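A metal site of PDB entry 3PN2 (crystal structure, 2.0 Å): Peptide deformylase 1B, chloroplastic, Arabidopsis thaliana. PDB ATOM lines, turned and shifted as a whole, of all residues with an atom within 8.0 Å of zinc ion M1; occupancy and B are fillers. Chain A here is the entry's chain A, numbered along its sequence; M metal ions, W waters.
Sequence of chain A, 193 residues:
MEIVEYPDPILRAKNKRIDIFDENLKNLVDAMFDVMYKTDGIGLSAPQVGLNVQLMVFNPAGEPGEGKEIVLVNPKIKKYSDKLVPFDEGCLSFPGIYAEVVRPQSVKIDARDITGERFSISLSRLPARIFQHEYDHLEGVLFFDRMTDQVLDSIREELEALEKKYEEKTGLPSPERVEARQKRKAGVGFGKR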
ATOM      1  N   VAL A   4     -26.443  13.280   2.174  1.00  0.00           N
ATOM      2  CA  VAL A   4     -27.387  12.297   1.620  1.00  0.00           C
ATOM      3  C   VAL A   4     -28.492  11.972   2.643  1.00  0.00           C
ATOM      4  O   VAL A   4     -28.200  11.688   3.773  1.00  0.00           O
ATOM      5  CB  VAL A   4     -26.618  11.032   1.213  1.00  0.00           C
ATOM      6  CG1 VAL A   4     -27.553   9.985   0.659  1.00  0.00           C
ATOM      7  CG2 VAL A   4     -25.552  11.425   0.141  1.00  0.00           C
ATOM      8  N   LEU A  11     -27.071   5.319   1.092  1.00  0.00           N
ATOM      9  CA  LEU A  11     -27.048   5.049   2.528  1.00  0.00           C
ATOM     10  C   LEU A  11     -27.192   3.576   2.833  1.00  0.00           C
ATOM     11  O   LEU A  11     -27.035   3.168   3.998  1.00  0.00           O
ATOM     12  CB  LEU A  11     -28.125   5.853   3.297  1.00  0.00           C
ATOM     13  CG  LEU A  11     -28.025   7.380   3.255  1.00  0.00           C
ATOM     14  CD1 LEU A  11     -29.245   7.967   3.834  1.00  0.00           C
ATOM     15  CD2 LEU A  11     -26.765   7.970   3.903  1.00  0.00           C
ATOM     16  N   GLY A  43     -19.186  12.879  14.897  1.00  0.00           N
ATOM     17  CA  GLY A  43     -18.725  11.923  13.856  1.00  0.00           C
ATOM     18  C   GLY A  43     -19.350  12.060  12.492  1.00  0.00           C
ATOM     19  O   GLY A  43     -20.467  12.593  12.340  1.00  0.00           O
ATOM     20  N   LEU A  44     -18.643  11.643  11.446  1.00  0.00           N
ATOM     21  CA  LEU A  44     -19.225  11.686  10.079  1.00  0.00           C
ATOM     22  C   LEU A  44     -18.595  10.621   9.197  1.00  0.00           C
ATOM     23  O   LEU A  44     -17.384  10.444   9.202  1.00  0.00           O
ATOM     24  CB  LEU A  44     -19.086  13.063   9.411  1.00  0.00           C
ATOM     25  CG  LEU A  44     -19.587  13.293   7.973  1.00  0.00           C
ATOM     26  CD1 LEU A  44     -20.983  12.979   7.888  1.00  0.00           C
ATOM     27  CD2 LEU A  44     -19.490  14.689   7.603  1.00  0.00           C
ATOM     28  N   SER A  45     -19.416   9.960   8.392  1.00  0.00           N
ATOM     29  CA  SER A  45     -19.021   8.780   7.638  1.00  0.00           C
ATOM     30  C   SER A  45     -19.106   9.133   6.165  1.00  0.00           C
ATOM     31  O   SER A  45     -19.898   9.969   5.777  1.00  0.00           O
ATOM     32  CB  SER A  45     -19.994   7.691   7.928  1.00  0.00           C
ATOM     33  OG  SER A  45     -21.252   8.079   7.354  1.00  0.00           O
ATOM     34  N   GLN A  48     -22.528   9.347   4.064  1.00  0.00           N
ATOM     35  CA  GLN A  48     -23.489  10.402   4.366  1.00  0.00           C
ATOM     36  C   GLN A  48     -23.222  11.625   3.538  1.00  0.00           C
ATOM     37  O   GLN A  48     -24.087  12.451   3.419  1.00  0.00           O
ATOM     38  CB  GLN A  48     -23.324  10.836   5.791  1.00  0.00           C
ATOM     39  CG  GLN A  48     -24.366  10.249   6.710  1.00  0.00           C
ATOM     40  CD  GLN A  48     -25.077  11.333   7.571  1.00  0.00           C
ATOM     41  OE1 GLN A  48     -24.476  12.366   7.923  1.00  0.00           O
ATOM     42  NE2 GLN A  48     -26.282  11.062   7.956  1.00  0.00           N
ATOM     43  N   GLU A  89     -31.552   9.719  19.699  1.00  0.00           N
ATOM     44  CA  GLU A  89     -30.649   9.932  18.581  1.00  0.00           C
ATOM     45  C   GLU A  89     -31.286  10.730  17.463  1.00  0.00           C
ATOM     46  O   GLU A  89     -32.487  10.664  17.241  1.00  0.00           O
ATOM     47  CB  GLU A  89     -30.255   8.581  18.007  1.00  0.00           C
ATOM     48  CG  GLU A  89     -28.995   8.157  18.540  1.00  0.00           C
ATOM     49  CD  GLU A  89     -28.685   6.754  18.130  1.00  0.00           C
ATOM     50  OE1 GLU A  89     -28.306   5.993  18.995  1.00  0.00           O
ATOM     51  OE2 GLU A  89     -28.807   6.445  16.936  1.00  0.00           O
ATOM     52  N   GLY A  90     -30.461  11.508  16.775  1.00  0.00           N
ATOM     53  CA  GLY A  90     -30.860  12.123  15.529  1.00  0.00           C
ATOM     54  C   GLY A  90     -29.937  11.540  14.474  1.00  0.00           C
ATOM     55  O   GLY A  90     -29.080  10.669  14.752  1.00  0.00           O
ATOM     56  N   CYS A  91     -30.023  12.083  13.284  1.00  0.00           N
ATOM     57  CA  CYS A  91     -29.223  11.611  12.181  1.00  0.00           C
ATOM     58  C   CYS A  91     -29.420  12.688  11.114  1.00  0.00           C
ATOM     59  O   CYS A  91     -30.549  13.048  10.777  1.00  0.00           O
ATOM     60  CB  CYS A  91     -29.762  10.296  11.641  1.00  0.00           C
ATOM     61  SG  CYS A  91     -28.824   9.777  10.169  1.00  0.00           S
ATOM     62  N   LEU A  92     -28.329  13.178  10.579  1.00  0.00           N
ATOM     63  CA  LEU A  92     -28.391  14.186   9.541  1.00  0.00           C
ATOM     64  C   LEU A  92     -29.134  13.722   8.283  1.00  0.00           C
ATOM     65  O   LEU A  92     -29.684  14.543   7.528  1.00  0.00           O
ATOM     66  CB  LEU A  92     -26.991  14.763   9.223  1.00  0.00           C
ATOM     67  CG  LEU A  92     -26.262  15.634  10.310  1.00  0.00           C
ATOM     68  CD1 LEU A  92     -24.893  16.025   9.661  1.00  0.00           C
ATOM     69  CD2 LEU A  92     -26.964  16.865  10.732  1.00  0.00           C
ATOM     70  N   SER A  93     -29.131  12.419   8.033  1.00  0.00           N
ATOM     71  CA  SER A  93     -29.868  11.851   6.835  1.00  0.00           C
ATOM     72  C   SER A  93     -31.374  11.821   7.011  1.00  0.00           C
ATOM     73  O   SER A  93     -32.089  11.482   6.058  1.00  0.00           O
ATOM     74  CB  SER A  93     -29.350  10.435   6.540  1.00  0.00           C
ATOM     75  OG  SER A  93     -27.952  10.546   6.215  1.00  0.00           O
ATOM     76  N   PHE A  94     -31.838  12.108   8.243  1.00  0.00           N
ATOM     77  CA  PHE A  94     -33.283  12.205   8.578  1.00  0.00           C
ATOM     78  C   PHE A  94     -33.531  13.550   9.248  1.00  0.00           C
ATOM     79  O   PHE A  94     -33.618  13.580  10.492  1.00  0.00           O
ATOM     80  CB  PHE A  94     -33.691  11.116   9.577  1.00  0.00           C
ATOM     81  CG  PHE A  94     -33.400   9.691   9.107  1.00  0.00           C
ATOM     82  CD1 PHE A  94     -32.104   9.205   9.046  1.00  0.00           C
ATOM     83  CD2 PHE A  94     -34.449   8.876   8.653  1.00  0.00           C
ATOM     84  CE1 PHE A  94     -31.862   7.936   8.596  1.00  0.00           C
ATOM     85  CE2 PHE A  94     -34.212   7.624   8.188  1.00  0.00           C
ATOM     86  CZ  PHE A  94     -32.927   7.131   8.157  1.00  0.00           C
ATOM     87  N   ARG A 103     -28.508   1.279  22.907  1.00  0.00           N
ATOM     88  CA  ARG A 103     -27.201   0.756  22.461  1.00  0.00           C
ATOM     89  C   ARG A 103     -26.307   0.354  23.609  1.00  0.00           C
ATOM     90  O   ARG A 103     -26.502   0.783  24.760  1.00  0.00           O
ATOM     91  CB  ARG A 103     -26.424   1.696  21.551  1.00  0.00           C
ATOM     92  CG  ARG A 103     -27.218   2.307  20.391  1.00  0.00           C
ATOM     93  CD  ARG A 103     -26.233   2.927  19.437  1.00  0.00           C
ATOM     94  NE  ARG A 103     -26.892   3.631  18.337  1.00  0.00           N
ATOM     95  CZ  ARG A 103     -26.941   3.236  17.084  1.00  0.00           C
ATOM     96  NH1 ARG A 103     -26.343   2.127  16.655  1.00  0.00           N
ATOM     97  NH2 ARG A 103     -27.612   3.990  16.218  1.00  0.00           N
ATOM     98  N   ILE A 130     -22.340   8.027  19.441  1.00  0.00           N
ATOM     99  CA  ILE A 130     -22.157   8.536  18.089  1.00  0.00           C
ATOM    100  C   ILE A 130     -21.295   7.592  17.246  1.00  0.00           C
ATOM    101  O   ILE A 130     -21.604   7.372  16.064  1.00  0.00           O
ATOM    102  CB  ILE A 130     -21.505   9.952  18.103  1.00  0.00           C
ATOM    103  CG1 ILE A 130     -22.333  10.921  18.963  1.00  0.00           C
ATOM    104  CG2 ILE A 130     -21.339  10.490  16.653  1.00  0.00           C
ATOM    105  CD1 ILE A 130     -23.887  11.083  18.592  1.00  0.00           C
ATOM    106  N   HIS A 133     -23.453   4.854  15.997  1.00  0.00           N
ATOM    107  CA  HIS A 133     -24.306   5.405  14.995  1.00  0.00           C
ATOM    108  C   HIS A 133     -23.565   5.597  13.632  1.00  0.00           C
ATOM    109  O   HIS A 133     -24.046   5.124  12.595  1.00  0.00           O
ATOM    110  CB  HIS A 133     -24.952   6.702  15.502  1.00  0.00           C
ATOM    111  CG  HIS A 133     -25.850   7.360  14.506  1.00  0.00           C
ATOM    112  ND1 HIS A 133     -27.201   7.476  14.706  1.00  0.00           N
ATOM    113  CD2 HIS A 133     -25.596   7.908  13.292  1.00  0.00           C
ATOM    114  CE1 HIS A 133     -27.756   8.091  13.672  1.00  0.00           C
ATOM    115  NE2 HIS A 133     -26.804   8.370  12.800  1.00  0.00           N
ATOM    116  N   GLU A 134     -22.457   6.324  13.616  1.00  0.00           N
ATOM    117  CA  GLU A 134     -21.703   6.482  12.376  1.00  0.00           C
ATOM    118  C   GLU A 134     -21.200   5.177  11.770  1.00  0.00           C
ATOM    119  O   GLU A 134     -21.166   5.057  10.572  1.00  0.00           O
ATOM    120  CB  GLU A 134     -20.526   7.426  12.560  1.00  0.00           C
ATOM    121  CG  GLU A 134     -20.924   8.799  12.848  1.00  0.00           C
ATOM    122  CD  GLU A 134     -21.955   9.244  11.856  1.00  0.00           C
ATOM    123  OE1 GLU A 134     -23.062   9.653  12.279  1.00  0.00           O
ATOM    124  OE2 GLU A 134     -21.684   9.140  10.632  1.00  0.00           O
ATOM    125  N   TYR A 135     -20.788   4.226  12.631  1.00  0.00           N
ATOM    126  CA  TYR A 135     -20.247   2.954  12.202  1.00  0.00           C
ATOM    127  C   TYR A 135     -21.306   2.128  11.518  1.00  0.00           C
ATOM    128  O   TYR A 135     -21.013   1.466  10.541  1.00  0.00           O
ATOM    129  CB  TYR A 135     -19.716   2.184  13.428  1.00  0.00           C
ATOM    130  CG  TYR A 135     -19.198   0.810  13.135  1.00  0.00           C
ATOM    131  CD1 TYR A 135     -19.934  -0.337  13.493  1.00  0.00           C
ATOM    132  CD2 TYR A 135     -17.939   0.625  12.548  1.00  0.00           C
ATOM    133  CE1 TYR A 135     -19.413  -1.638  13.245  1.00  0.00           C
ATOM    134  CE2 TYR A 135     -17.426  -0.644  12.318  1.00  0.00           C
ATOM    135  CZ  TYR A 135     -18.164  -1.769  12.668  1.00  0.00           C
ATOM    136  OH  TYR A 135     -17.621  -3.007  12.421  1.00  0.00           O
ATOM    137  N   ASP A 136     -22.528   2.194  12.040  1.00  0.00           N
ATOM    138  CA  ASP A 136     -23.706   1.648  11.345  1.00  0.00           C
ATOM    139  C   ASP A 136     -23.792   2.177   9.905  1.00  0.00           C
ATOM    140  O   ASP A 136     -23.954   1.397   8.981  1.00  0.00           O
ATOM    141  CB  ASP A 136     -25.010   1.945  12.121  1.00  0.00           C
ATOM    142  CG  ASP A 136     -25.244   1.035  13.300  1.00  0.00           C
ATOM    143  OD1 ASP A 136     -26.246   1.228  14.017  1.00  0.00           O
ATOM    144  OD2 ASP A 136     -24.452   0.110  13.532  1.00  0.00           O
ATOM    145  N   HIS A 137     -23.680   3.503   9.694  1.00  0.00           N
ATOM    146  CA  HIS A 137     -23.677   3.994   8.307  1.00  0.00           C
ATOM    147  C   HIS A 137     -22.725   3.193   7.402  1.00  0.00           C
ATOM    148  O   HIS A 137     -23.065   2.901   6.266  1.00  0.00           O
ATOM    149  CB  HIS A 137     -23.327   5.446   8.234  1.00  0.00           C
ATOM    150  CG  HIS A 137     -24.464   6.347   8.608  1.00  0.00           C
ATOM    151  ND1 HIS A 137     -25.623   6.410   7.870  1.00  0.00           N
ATOM    152  CD2 HIS A 137     -24.642   7.168   9.664  1.00  0.00           C
ATOM    153  CE1 HIS A 137     -26.452   7.280   8.431  1.00  0.00           C
ATOM    154  NE2 HIS A 137     -25.887   7.733   9.536  1.00  0.00           N
ATOM    155  N   VAL A 141     -26.461   0.363   7.693  1.00  0.00           N
ATOM    156  CA  VAL A 141     -27.481   0.243   8.748  1.00  0.00           C
ATOM    157  C   VAL A 141     -27.861   1.663   9.117  1.00  0.00           C
ATOM    158  O   VAL A 141     -26.996   2.524   9.221  1.00  0.00           O
ATOM    159  CB  VAL A 141     -26.959  -0.527   9.963  1.00  0.00           C
ATOM    160  CG1 VAL A 141     -27.892  -0.366  11.125  1.00  0.00           C
ATOM    161  CG2 VAL A 141     -26.787  -2.040   9.668  1.00  0.00           C
ATOM    162  N   LEU A 142     -29.171   1.904   9.272  1.00  0.00           N
ATOM    163  CA  LEU A 142     -29.691   3.214   9.586  1.00  0.00           C
ATOM    164  C   LEU A 142     -30.407   3.080  10.936  1.00  0.00           C
ATOM    165  O   LEU A 142     -30.770   1.984  11.326  1.00  0.00           O
ATOM    166  CB  LEU A 142     -30.609   3.753   8.462  1.00  0.00           C
ATOM    167  CG  LEU A 142     -29.997   3.857   7.062  1.00  0.00           C
ATOM    168  CD1 LEU A 142     -31.012   4.435   6.076  1.00  0.00           C
ATOM    169  CD2 LEU A 142     -28.785   4.702   7.020  1.00  0.00           C
ATOM    170  N   PHE A 143     -30.552   4.196  11.680  1.00  0.00           N
ATOM    171  CA  PHE A 143     -30.875   4.146  13.140  1.00  0.00           C
ATOM    172  C   PHE A 143     -32.262   3.575  13.475  1.00  0.00           C
ATOM    173  O   PHE A 143     -32.455   2.900  14.525  1.00  0.00           O
ATOM    174  CB  PHE A 143     -30.494   5.485  13.884  1.00  0.00           C
ATOM    175  CG  PHE A 143     -31.464   6.673  13.677  1.00  0.00           C
ATOM    176  CD1 PHE A 143     -31.735   7.538  14.724  1.00  0.00           C
ATOM    177  CD2 PHE A 143     -32.069   6.910  12.431  1.00  0.00           C
ATOM    178  CE1 PHE A 143     -32.611   8.629  14.582  1.00  0.00           C
ATOM    179  CE2 PHE A 143     -32.956   7.969  12.251  1.00  0.00           C
ATOM    180  CZ  PHE A 143     -33.215   8.874  13.326  1.00  0.00           C
HETATM  181 ZN    ZN M   1     -26.877   9.052  10.927  1.00  0.00          ZN
HETATM  182 ZN    ZN M   2     -23.604  10.598  10.037  1.00  0.00          ZN
HETATM  183  O   HOH W   1     -25.613  10.303  10.787  1.00  0.00           O
HETATM  184  O   HOH W   2     -29.005   6.467  10.683  1.00  0.00           O
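A ring nitrogen (ND1) of His 133 sits at hydrogen-bond distance from the side-chain carboxylate (OE2) of Glu 89, 2.9 Å away.
SG of Cys 91 sits close to NE2 of Gln 48 (3.6 Å).
SG of Cys 91 lies close to N of Ser 93.
The side-chain amide nitrogen (NE2) of Gln 48 is in hydrogen-bond range of the side-chain hydroxyl (OG) of Ser 93.
The backbone carbonyl oxygen (O) of Gln 48 is in hydrogen-bond range of the backbone NH (N) of Val 4 (2.8 Å).
Gln 48 touches zinc ion M1.
Four residues have an atom within 4 Å of zinc ion M1: Gln 48, Cys 91, His 133 and His 137.
Along chain A the residues within 4 Å of zinc ion M1 span positions 48 to 137.
Water W1 binds zinc ion M1, at 1.8 Å.
NE2 of His 133 is bound to zinc ion M1 (2.0 Å).
Zinc ion M1 is bound by NE2 of His 137.
SG of Cys 91 is bound to zinc ion M1, at 2.2 Å.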
